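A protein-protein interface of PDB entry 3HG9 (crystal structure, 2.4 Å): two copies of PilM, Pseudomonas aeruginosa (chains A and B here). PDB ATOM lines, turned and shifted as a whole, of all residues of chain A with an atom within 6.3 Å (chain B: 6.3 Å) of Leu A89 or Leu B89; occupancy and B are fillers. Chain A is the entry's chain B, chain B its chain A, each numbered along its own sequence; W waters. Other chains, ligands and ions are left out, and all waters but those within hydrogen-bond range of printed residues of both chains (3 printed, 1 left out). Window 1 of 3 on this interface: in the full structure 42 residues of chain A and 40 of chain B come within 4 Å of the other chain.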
ATOM      1  N   ARG A  23      37.495  -2.173  17.061  1.00  0.00           N
ATOM      2  CA  ARG A  23      36.071  -2.377  17.248  1.00  0.00           C
ATOM      3  C   ARG A  23      35.704  -3.861  17.447  1.00  0.00           C
ATOM      4  O   ARG A  23      34.911  -4.237  18.352  1.00  0.00           O
ATOM      5  CB  ARG A  23      35.242  -1.795  16.073  1.00  0.00           C
ATOM      6  CG  ARG A  23      33.726  -1.845  16.406  1.00  0.00           C
ATOM      7  CD  ARG A  23      32.857  -1.235  15.375  1.00  0.00           C
ATOM      8  NE  ARG A  23      32.539  -2.178  14.296  1.00  0.00           N
ATOM      9  CZ  ARG A  23      31.641  -1.946  13.338  1.00  0.00           C
ATOM     10  NH1 ARG A  23      30.975  -0.801  13.357  1.00  0.00           N
ATOM     11  NH2 ARG A  23      31.417  -2.850  12.347  1.00  0.00           N
ATOM     12  N   THR A  85      32.857  -1.047   6.272  1.00  0.00           N
ATOM     13  CA  THR A  85      31.955  -1.625   7.292  1.00  0.00           C
ATOM     14  C   THR A  85      30.824  -2.478   6.700  1.00  0.00           C
ATOM     15  O   THR A  85      30.739  -3.667   6.998  1.00  0.00           O
ATOM     16  CB  THR A  85      31.394  -0.557   8.287  1.00  0.00           C
ATOM     17  OG1 THR A  85      30.995   0.618   7.576  1.00  0.00           O
ATOM     18  CG2 THR A  85      32.466  -0.154   9.322  1.00  0.00           C
ATOM     19  N   SER A  87      26.993  -2.437   7.036  1.00  0.00           N
ATOM     20  CA  SER A  87      25.920  -1.791   7.787  1.00  0.00           C
ATOM     21  C   SER A  87      24.712  -2.690   7.829  1.00  0.00           C
ATOM     22  O   SER A  87      24.449  -3.449   6.883  1.00  0.00           O
ATOM     23  CB  SER A  87      25.541  -0.429   7.199  1.00  0.00           C
ATOM     24  OG  SER A  87      24.963   0.445   8.190  1.00  0.00           O
ATOM     25  N   ASP A  88      23.984  -2.643   8.941  1.00  0.00           N
ATOM     26  CA  ASP A  88      23.000  -3.698   9.155  1.00  0.00           C
ATOM     27  C   ASP A  88      21.982  -3.245  10.110  1.00  0.00           C
ATOM     28  O   ASP A  88      22.319  -2.991  11.291  1.00  0.00           O
ATOM     29  CB  ASP A  88      23.659  -4.973   9.704  1.00  0.00           C
ATOM     30  CG  ASP A  88      22.622  -6.099  10.051  1.00  0.00           C
ATOM     31  OD1 ASP A  88      23.022  -7.313   9.933  1.00  0.00           O
ATOM     32  OD2 ASP A  88      21.443  -5.771  10.471  1.00  0.00           O
ATOM     33  N   LEU A  89      20.749  -3.148   9.605  1.00  0.00           N
ATOM     34  CA  LEU A  89      19.587  -2.740  10.408  1.00  0.00           C
ATOM     35  C   LEU A  89      18.489  -3.703  10.171  1.00  0.00           C
ATOM     36  O   LEU A  89      18.533  -4.453   9.199  1.00  0.00           O
ATOM     37  CB  LEU A  89      19.084  -1.358  10.022  1.00  0.00           C
ATOM     38  CG  LEU A  89      20.247  -0.429   9.764  1.00  0.00           C
ATOM     39  CD1 LEU A  89      19.913   0.624   8.707  1.00  0.00           C
ATOM     40  CD2 LEU A  89      20.800   0.123  11.098  1.00  0.00           C
ATOM     41  N   VAL A  90      17.511  -3.696  11.064  1.00  0.00           N
ATOM     42  CA  VAL A  90      16.238  -4.351  10.826  1.00  0.00           C
ATOM     43  C   VAL A  90      15.199  -3.429  11.405  1.00  0.00           C
ATOM     44  O   VAL A  90      15.511  -2.668  12.321  1.00  0.00           O
ATOM     45  CB  VAL A  90      16.133  -5.760  11.497  1.00  0.00           C
ATOM     46  CG1 VAL A  90      17.279  -6.695  11.046  1.00  0.00           C
ATOM     47  CG2 VAL A  90      16.073  -5.663  12.992  1.00  0.00           C
ATOM     48  N   GLY A  91      13.975  -3.498  10.905  1.00  0.00           N
ATOM     49  CA  GLY A  91      12.873  -2.777  11.523  1.00  0.00           C
ATOM     50  C   GLY A  91      11.687  -2.769  10.559  1.00  0.00           C
ATOM     51  O   GLY A  91      11.797  -3.233   9.416  1.00  0.00           O
ATOM     52  N   LEU A  98      12.113   3.292   8.402  1.00  0.00           N
ATOM     53  CA  LEU A  98      12.405   1.990   8.996  1.00  0.00           C
ATOM     54  C   LEU A  98      12.498   2.110  10.496  1.00  0.00           C
ATOM     55  O   LEU A  98      13.510   2.529  11.042  1.00  0.00           O
ATOM     56  CB  LEU A  98      13.724   1.433   8.477  1.00  0.00           C
ATOM     57  CG  LEU A  98      14.081   0.011   8.908  1.00  0.00           C
ATOM     58  CD1 LEU A  98      13.208  -0.846   8.078  1.00  0.00           C
ATOM     59  CD2 LEU A  98      15.596  -0.400   8.735  1.00  0.00           C
ATOM     60  N   THR A 100      13.290   1.060  13.881  1.00  0.00           N
ATOM     61  CA  THR A 100      13.928   0.065  14.773  1.00  0.00           C
ATOM     62  C   THR A 100      14.005   0.445  16.248  1.00  0.00           C
ATOM     63  O   THR A 100      14.823   1.299  16.627  1.00  0.00           O
ATOM     64  CB  THR A 100      15.346  -0.316  14.332  1.00  0.00           C
ATOM     65  OG1 THR A 100      16.085  -0.755  15.486  1.00  0.00           O
ATOM     66  CG2 THR A 100      16.072   0.872  13.684  1.00  0.00           C
ATOM     67  N   LEU A 103      17.081   2.416  17.910  1.00  0.00           N
ATOM     68  CA  LEU A 103      17.657   3.547  17.197  1.00  0.00           C
ATOM     69  C   LEU A 103      16.563   4.408  16.563  1.00  0.00           C
ATOM     70  O   LEU A 103      16.841   5.194  15.654  1.00  0.00           O
ATOM     71  CB  LEU A 103      18.683   3.058  16.157  1.00  0.00           C
ATOM     72  CG  LEU A 103      19.802   2.071  16.597  1.00  0.00           C
ATOM     73  CD1 LEU A 103      20.246   2.237  18.115  1.00  0.00           C
ATOM     74  CD2 LEU A 103      19.433   0.640  16.310  1.00  0.00           C
ATOM     75  N   THR A 106      14.598   5.247  11.441  1.00  0.00           N
ATOM     76  CA  THR A 106      15.717   5.576  10.584  1.00  0.00           C
ATOM     77  C   THR A 106      15.188   5.703   9.137  1.00  0.00           C
ATOM     78  O   THR A 106      14.648   4.731   8.550  1.00  0.00           O
ATOM     79  CB  THR A 106      16.879   4.521  10.726  1.00  0.00           C
ATOM     80  OG1 THR A 106      16.513   3.283  10.098  1.00  0.00           O
ATOM     81  CG2 THR A 106      17.189   4.190  12.162  1.00  0.00           C
ATOM     82  N   ILE A 108      14.995   5.959   5.297  1.00  0.00           N
ATOM     83  CA  ILE A 108      15.749   5.413   4.139  1.00  0.00           C
ATOM     84  C   ILE A 108      15.095   5.436   2.718  1.00  0.00           C
ATOM     85  O   ILE A 108      13.854   5.426   2.570  1.00  0.00           O
ATOM     86  CB  ILE A 108      16.227   3.942   4.361  1.00  0.00           C
ATOM     87  CG1 ILE A 108      16.403   3.588   5.821  1.00  0.00           C
ATOM     88  CG2 ILE A 108      17.476   3.616   3.503  1.00  0.00           C
ATOM     89  CD1 ILE A 108      16.528   2.091   5.973  1.00  0.00           C
ATOM     90  N   VAL A 120      11.743  -5.963   7.810  1.00  0.00           N
ATOM     91  CA  VAL A 120      12.830  -5.792   6.835  1.00  0.00           C
ATOM     92  C   VAL A 120      14.266  -5.962   7.405  1.00  0.00           C
ATOM     93  O   VAL A 120      14.687  -5.247   8.331  1.00  0.00           O
ATOM     94  CB  VAL A 120      12.877  -4.323   6.282  1.00  0.00           C
ATOM     95  CG1 VAL A 120      13.477  -4.292   4.866  1.00  0.00           C
ATOM     96  CG2 VAL A 120      11.536  -3.621   6.317  1.00  0.00           C
ATOM     97  N   ALA A 121      15.073  -6.805   6.792  1.00  0.00           N
ATOM     98  CA  ALA A 121      16.470  -6.842   7.160  1.00  0.00           C
ATOM     99  C   ALA A 121      17.320  -6.229   6.085  1.00  0.00           C
ATOM    100  O   ALA A 121      17.231  -6.644   4.905  1.00  0.00           O
ATOM    101  CB  ALA A 121      16.923  -8.279   7.377  1.00  0.00           C
ATOM    102  N   VAL A 122      18.178  -5.287   6.495  1.00  0.00           N
ATOM    103  CA  VAL A 122      18.913  -4.445   5.572  1.00  0.00           C
ATOM    104  C   VAL A 122      20.394  -4.662   5.726  1.00  0.00           C
ATOM    105  O   VAL A 122      20.941  -4.553   6.806  1.00  0.00           O
ATOM    106  CB  VAL A 122      18.581  -2.930   5.809  1.00  0.00           C
ATOM    107  CG1 VAL A 122      19.273  -2.031   4.756  1.00  0.00           C
ATOM    108  CG2 VAL A 122      17.061  -2.663   5.812  1.00  0.00           C
ATOM    109  N   LYS A 123      21.084  -4.952   4.649  1.00  0.00           N
ATOM    110  CA  LYS A 123      22.478  -5.295   4.769  1.00  0.00           C
ATOM    111  C   LYS A 123      23.158  -4.476   3.708  1.00  0.00           C
ATOM    112  O   LYS A 123      23.306  -4.948   2.561  1.00  0.00           O
ATOM    113  CB  LYS A 123      22.686  -6.799   4.505  1.00  0.00           C
ATOM    114  CG  LYS A 123      24.138  -7.273   4.236  1.00  0.00           C
ATOM    115  CD  LYS A 123      24.819  -7.793   5.472  1.00  0.00           C
ATOM    116  CE  LYS A 123      25.437  -9.176   5.258  1.00  0.00           C
ATOM    117  NZ  LYS A 123      24.334 -10.190   5.334  1.00  0.00           N
ATOM    118  N   GLU A 124      23.569  -3.251   4.043  1.00  0.00           N
ATOM    119  CA  GLU A 124      24.288  -2.527   3.010  1.00  0.00           C
ATOM    120  C   GLU A 124      25.453  -3.374   2.358  1.00  0.00           C
ATOM    121  O   GLU A 124      26.102  -4.231   2.987  1.00  0.00           O
ATOM    122  CB  GLU A 124      24.651  -1.100   3.408  1.00  0.00           C
ATOM    123  CG  GLU A 124      24.295  -0.046   2.298  1.00  0.00           C
ATOM    124  CD  GLU A 124      25.179   1.263   2.299  1.00  0.00           C
ATOM    125  OE1 GLU A 124      26.451   1.166   2.379  1.00  0.00           O
ATOM    126  OE2 GLU A 124      24.578   2.389   2.193  1.00  0.00           O
ATOM    127  N   ARG B  23      18.568 -13.246   3.810  1.00  0.00           N
ATOM    128  CA  ARG B  23      19.325 -12.011   3.571  1.00  0.00           C
ATOM    129  C   ARG B  23      20.834 -12.252   3.297  1.00  0.00           C
ATOM    130  O   ARG B  23      21.445 -11.600   2.419  1.00  0.00           O
ATOM    131  CB  ARG B  23      19.125 -10.993   4.685  1.00  0.00           C
ATOM    132  CG  ARG B  23      19.829  -9.661   4.381  1.00  0.00           C
ATOM    133  CD  ARG B  23      19.861  -8.789   5.574  1.00  0.00           C
ATOM    134  NE  ARG B  23      20.775  -9.290   6.625  1.00  0.00           N
ATOM    135  CZ  ARG B  23      20.946  -8.704   7.810  1.00  0.00           C
ATOM    136  NH1 ARG B  23      20.254  -7.577   8.073  1.00  0.00           N
ATOM    137  NH2 ARG B  23      21.784  -9.259   8.739  1.00  0.00           N
ATOM    138  N   THR B  85      19.908 -10.522  14.888  1.00  0.00           N
ATOM    139  CA  THR B  85      20.870  -9.661  14.175  1.00  0.00           C
ATOM    140  C   THR B  85      21.634  -8.780  15.146  1.00  0.00           C
ATOM    141  O   THR B  85      21.215  -8.562  16.305  1.00  0.00           O
ATOM    142  CB  THR B  85      20.208  -8.645  13.241  1.00  0.00           C
ATOM    143  OG1 THR B  85      19.065  -8.087  13.890  1.00  0.00           O
ATOM    144  CG2 THR B  85      19.796  -9.270  11.943  1.00  0.00           C
ATOM    145  N   SER B  87      23.471  -5.248  14.166  1.00  0.00           N
ATOM    146  CA  SER B  87      23.257  -3.830  13.827  1.00  0.00           C
ATOM    147  C   SER B  87      24.616  -3.159  13.931  1.00  0.00           C
ATOM    148  O   SER B  87      25.435  -3.475  14.815  1.00  0.00           O
ATOM    149  CB  SER B  87      22.140  -3.145  14.650  1.00  0.00           C
ATOM    150  OG  SER B  87      20.849  -3.728  14.358  1.00  0.00           O
ATOM    151  N   ASP B  88      24.900  -2.312  12.949  1.00  0.00           N
ATOM    152  CA  ASP B  88      26.274  -1.906  12.744  1.00  0.00           C
ATOM    153  C   ASP B  88      26.169  -0.676  11.960  1.00  0.00           C
ATOM    154  O   ASP B  88      25.674  -0.738  10.839  1.00  0.00           O
ATOM    155  CB  ASP B  88      27.029  -2.966  11.912  1.00  0.00           C
ATOM    156  CG  ASP B  88      28.247  -2.386  11.124  1.00  0.00           C
ATOM    157  OD1 ASP B  88      29.176  -3.194  10.774  1.00  0.00           O
ATOM    158  OD2 ASP B  88      28.259  -1.139  10.859  1.00  0.00           O
ATOM    159  N   LEU B  89      26.640   0.420  12.541  1.00  0.00           N
ATOM    160  CA  LEU B  89      26.586   1.711  11.896  1.00  0.00           C
ATOM    161  C   LEU B  89      27.865   2.460  12.021  1.00  0.00           C
ATOM    162  O   LEU B  89      28.723   2.107  12.863  1.00  0.00           O
ATOM    163  CB  LEU B  89      25.545   2.598  12.523  1.00  0.00           C
ATOM    164  CG  LEU B  89      24.155   2.116  12.261  1.00  0.00           C
ATOM    165  CD1 LEU B  89      23.644   1.352  13.578  1.00  0.00           C
ATOM    166  CD2 LEU B  89      23.439   3.322  11.935  1.00  0.00           C
ATOM    167  N   VAL B  90      27.975   3.499  11.190  1.00  0.00           N
ATOM    168  CA  VAL B  90      29.095   4.423  11.194  1.00  0.00           C
ATOM    169  C   VAL B  90      28.580   5.870  11.079  1.00  0.00           C
ATOM    170  O   VAL B  90      27.717   6.157  10.204  1.00  0.00           O
ATOM    171  CB  VAL B  90      30.090   4.040  10.053  1.00  0.00           C
ATOM    172  CG1 VAL B  90      31.161   5.083   9.846  1.00  0.00           C
ATOM    173  CG2 VAL B  90      30.762   2.709  10.402  1.00  0.00           C
ATOM    174  N   GLY B  91      29.093   6.771  11.923  1.00  0.00           N
ATOM    175  CA  GLY B  91      29.031   8.217  11.595  1.00  0.00           C
ATOM    176  C   GLY B  91      29.827   9.163  12.508  1.00  0.00           C
ATOM    177  O   GLY B  91      30.934   8.832  12.960  1.00  0.00           O
ATOM    178  N   LEU B  98      23.720  10.299  15.960  1.00  0.00           N
ATOM    179  CA  LEU B  98      24.747   9.841  15.010  1.00  0.00           C
ATOM    180  C   LEU B  98      24.459  10.309  13.613  1.00  0.00           C
ATOM    181  O   LEU B  98      23.380  10.087  13.102  1.00  0.00           O
ATOM    182  CB  LEU B  98      24.856   8.318  14.986  1.00  0.00           C
ATOM    183  CG  LEU B  98      26.057   7.750  14.246  1.00  0.00           C
ATOM    184  CD1 LEU B  98      27.256   8.168  15.059  1.00  0.00           C
ATOM    185  CD2 LEU B  98      25.969   6.209  14.106  1.00  0.00           C
ATOM    186  N   THR B 100      25.117   9.974   9.844  1.00  0.00           N
ATOM    187  CA  THR B 100      25.728   9.073   8.908  1.00  0.00           C
ATOM    188  C   THR B 100      25.261   9.292   7.473  1.00  0.00           C
ATOM    189  O   THR B 100      24.043   9.397   7.182  1.00  0.00           O
ATOM    190  CB  THR B 100      25.516   7.641   9.349  1.00  0.00           C
ATOM    191  OG1 THR B 100      26.089   6.775   8.364  1.00  0.00           O
ATOM    192  CG2 THR B 100      24.024   7.345   9.556  1.00  0.00           C
ATOM    193  N   LEU B 103      22.254   7.642   5.113  1.00  0.00           N
ATOM    194  CA  LEU B 103      21.302   7.143   6.125  1.00  0.00           C
ATOM    195  C   LEU B 103      20.636   8.212   7.026  1.00  0.00           C
ATOM    196  O   LEU B 103      19.827   7.877   7.919  1.00  0.00           O
ATOM    197  CB  LEU B 103      21.950   6.051   6.978  1.00  0.00           C
ATOM    198  CG  LEU B 103      21.875   4.583   6.513  1.00  0.00           C
ATOM    199  CD1 LEU B 103      22.616   4.281   5.194  1.00  0.00           C
ATOM    200  CD2 LEU B 103      22.321   3.621   7.614  1.00  0.00           C
ATOM    201  N   THR B 106      20.711   9.440  12.889  1.00  0.00           N
ATOM    202  CA  THR B 106      20.064   8.396  13.709  1.00  0.00           C
ATOM    203  C   THR B 106      20.242   8.780  15.219  1.00  0.00           C
ATOM    204  O   THR B 106      21.373   9.107  15.646  1.00  0.00           O
ATOM    205  CB  THR B 106      20.673   6.936  13.428  1.00  0.00           C
ATOM    206  OG1 THR B 106      21.967   6.784  14.057  1.00  0.00           O
ATOM    207  CG2 THR B 106      20.804   6.580  11.904  1.00  0.00           C
ATOM    208  N   ILE B 108      20.827   7.350  18.504  1.00  0.00           N
ATOM    209  CA  ILE B 108      21.219   6.335  19.467  1.00  0.00           C
ATOM    210  C   ILE B 108      21.608   7.091  20.722  1.00  0.00           C
ATOM    211  O   ILE B 108      21.969   8.281  20.653  1.00  0.00           O
ATOM    212  CB  ILE B 108      22.524   5.630  19.062  1.00  0.00           C
ATOM    213  CG1 ILE B 108      22.668   5.573  17.555  1.00  0.00           C
ATOM    214  CG2 ILE B 108      22.686   4.238  19.731  1.00  0.00           C
ATOM    215  CD1 ILE B 108      23.924   4.829  17.109  1.00  0.00           C
ATOM    216  N   VAL B 120      32.783   7.497  14.788  1.00  0.00           N
ATOM    217  CA  VAL B 120      32.226   6.409  15.655  1.00  0.00           C
ATOM    218  C   VAL B 120      31.639   5.225  14.873  1.00  0.00           C
ATOM    219  O   VAL B 120      30.680   5.398  14.073  1.00  0.00           O
ATOM    220  CB  VAL B 120      30.946   6.834  16.404  1.00  0.00           C
ATOM    221  CG1 VAL B 120      30.594   5.822  17.471  1.00  0.00           C
ATOM    222  CG2 VAL B 120      31.052   8.232  16.987  1.00  0.00           C
ATOM    223  N   ALA B 121      32.160   4.024  15.096  1.00  0.00           N
ATOM    224  CA  ALA B 121      31.467   2.919  14.572  1.00  0.00           C
ATOM    225  C   ALA B 121      30.830   2.189  15.711  1.00  0.00           C
ATOM    226  O   ALA B 121      31.481   2.005  16.750  1.00  0.00           O
ATOM    227  CB  ALA B 121      32.429   2.060  13.863  1.00  0.00           C
ATOM    228  N   VAL B 122      29.586   1.727  15.515  1.00  0.00           N
ATOM    229  CA  VAL B 122      28.865   0.991  16.565  1.00  0.00           C
ATOM    230  C   VAL B 122      28.627  -0.469  16.210  1.00  0.00           C
ATOM    231  O   VAL B 122      28.426  -0.747  15.063  1.00  0.00           O
ATOM    232  CB  VAL B 122      27.490   1.616  16.792  1.00  0.00           C
ATOM    233  CG1 VAL B 122      26.782   0.937  17.990  1.00  0.00           C
ATOM    234  CG2 VAL B 122      27.597   3.161  16.979  1.00  0.00           C
ATOM    235  N   LYS B 123      28.625  -1.393  17.171  1.00  0.00           N
ATOM    236  CA  LYS B 123      28.091  -2.766  16.953  1.00  0.00           C
ATOM    237  C   LYS B 123      27.405  -3.355  18.178  1.00  0.00           C
ATOM    238  O   LYS B 123      27.938  -3.290  19.279  1.00  0.00           O
ATOM    239  CB  LYS B 123      29.174  -3.762  16.515  1.00  0.00           C
ATOM    240  CG  LYS B 123      28.635  -4.896  15.591  1.00  0.00           C
ATOM    241  CD  LYS B 123      29.487  -6.127  15.583  1.00  0.00           C
ATOM    242  CE  LYS B 123      29.142  -6.968  14.361  1.00  0.00           C
ATOM    243  NZ  LYS B 123      30.220  -7.013  13.305  1.00  0.00           N
ATOM    244  N   GLU B 124      26.237  -3.957  17.971  1.00  0.00           N
ATOM    245  CA  GLU B 124      25.465  -4.632  19.036  1.00  0.00           C
ATOM    246  C   GLU B 124      25.822  -6.116  19.213  1.00  0.00           C
ATOM    247  O   GLU B 124      26.757  -6.576  18.583  1.00  0.00           O
ATOM    248  CB  GLU B 124      23.990  -4.432  18.727  1.00  0.00           C
ATOM    249  CG  GLU B 124      23.649  -2.913  18.474  1.00  0.00           C
ATOM    250  CD  GLU B 124      22.124  -2.613  18.352  1.00  0.00           C
ATOM    251  OE1 GLU B 124      21.331  -3.571  18.093  1.00  0.00           O
ATOM    252  OE2 GLU B 124      21.736  -1.418  18.507  1.00  0.00           O
HETATM  253  O   HOH W   1      22.558 -11.508   6.862  1.00  0.00           O
HETATM  254  O   HOH W   2      18.635  -2.400  13.807  1.00  0.00           O
HETATM  255  O   HOH W   3      30.099  -4.742   9.169  1.00  0.00           O
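The guanidinium group (NH2) of Arg B23 is in salt-bridge range of the side-chain carboxylate (OD1) of Asp A88, 2.6 Å away.
The guanidinium group (NH1) of Arg B23 sits at hydrogen-bond distance from the backbone carbonyl oxygen (O) of Val A122, at 3.3 Å.
O of Asp A88 lies close to OG of Ser B87, at 3.5 Å.
The guanidinium group (NH2) of Arg A23 is in salt-bridge range of the side-chain carboxylate (OD1) of Asp B88 (2.8 Å).
O of Asp B88 lies within hydrogen-bond range of OG of Ser A87, at 3.0 Å.
N of Asp B88 is in hydrogen-bond range of O of Asp A88, at 3.1 Å.
The guanidinium group of Arg A23 sits at hydrogen-bond distance from the backbone carbonyl oxygen of Val B122.
O of Ser B87 sits at hydrogen-bond distance from N of Glu B124 (3.3 Å).
The backbone carbonyl oxygen of Leu B89 lies within hydrogen-bond range of the backbone NH of Val B122 (2.8 Å).
The backbone carbonyl oxygen (O) of Val B90 sits at hydrogen-bond distance from the side-chain hydroxyl (OG1) of Thr B100, at 2.5 Å.
The backbone NH (N) of Glu A124 lies within hydrogen-bond range of the backbone carbonyl oxygen (O) of Ser A87, at 3.0 Å.
The backbone NH (N) of Val A122 is in hydrogen-bond range of the backbone carbonyl oxygen (O) of Leu A89 (2.9 Å).
Among the printed residues, pairs that only touch across the chains: Arg A23 with Ala B121, Ala A121 with Arg B23, Thr A85 with Val B90, Leu A103 with Ile B108, Lys A123 with Arg B23, Val A90 with Thr B85, Arg A23 with Leu B89, Leu A89 with Arg B23, Leu A103 with Glu B124, Leu A89 with Leu B89 and Leu A89 with Leu B103.
Of the printed residues of chain B, Thr A85 touches Val B90.
Printed residues of chain B within 4 Å of Ser A87: Asp B88 (3.0 Å).
Printed residues of chain B within 4 Å of Leu A89: Arg B23 (3.7 Å), Leu B89 (3.97 Å) and Leu B103 (3.997 Å).
Gly A91 touches none of the printed residues of chain B.
Printed residues of chain A within 4 Å of Ser B87: Asp A88 (2.8 Å).
Leu B89 touches just these residues of chain A: Arg A23 (3.7 Å) and Leu A89 (3.97 Å).
Thr B100 touches none of the printed residues of chain A.
Of the 17 printed residues of chain A, 10 touch a printed residue of chain B.
Hydrophobic or aromatic side chains of chain A that line the printed part of chain B: Leu A89, Val A90, Leu A103 and Ala A121.
Among the printed residues, 18 pairs touch across the chains.
Arg A23 touches Asp B88, and with the chains exchanged Asp A88 touches Arg B23.
Arg A23 touches Ala B121, and with the chains exchanged Ala A121 touches Arg B23.
Thr A85 touches Val B90, and with the chains exchanged Val A90 touches Thr B85.
Leu A89 touches its own counterpart, Leu B89.
17 positions are printed for both chains.
Water W3 lies within hydrogen-bond range of OD1 of Asp B88 (2.4 Å) and O of Thr A85 (2.5 Å).
Water W2 lies within hydrogen-bond range of the side-chain hydroxyl of Ser B87 (2.6 Å), the backbone NH of Val A90 (3.2 Å) and the side-chain hydroxyl of Thr A100 (3.5 Å).
Water W1 bridges NZ of Lys A123 and NE of Arg B23.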
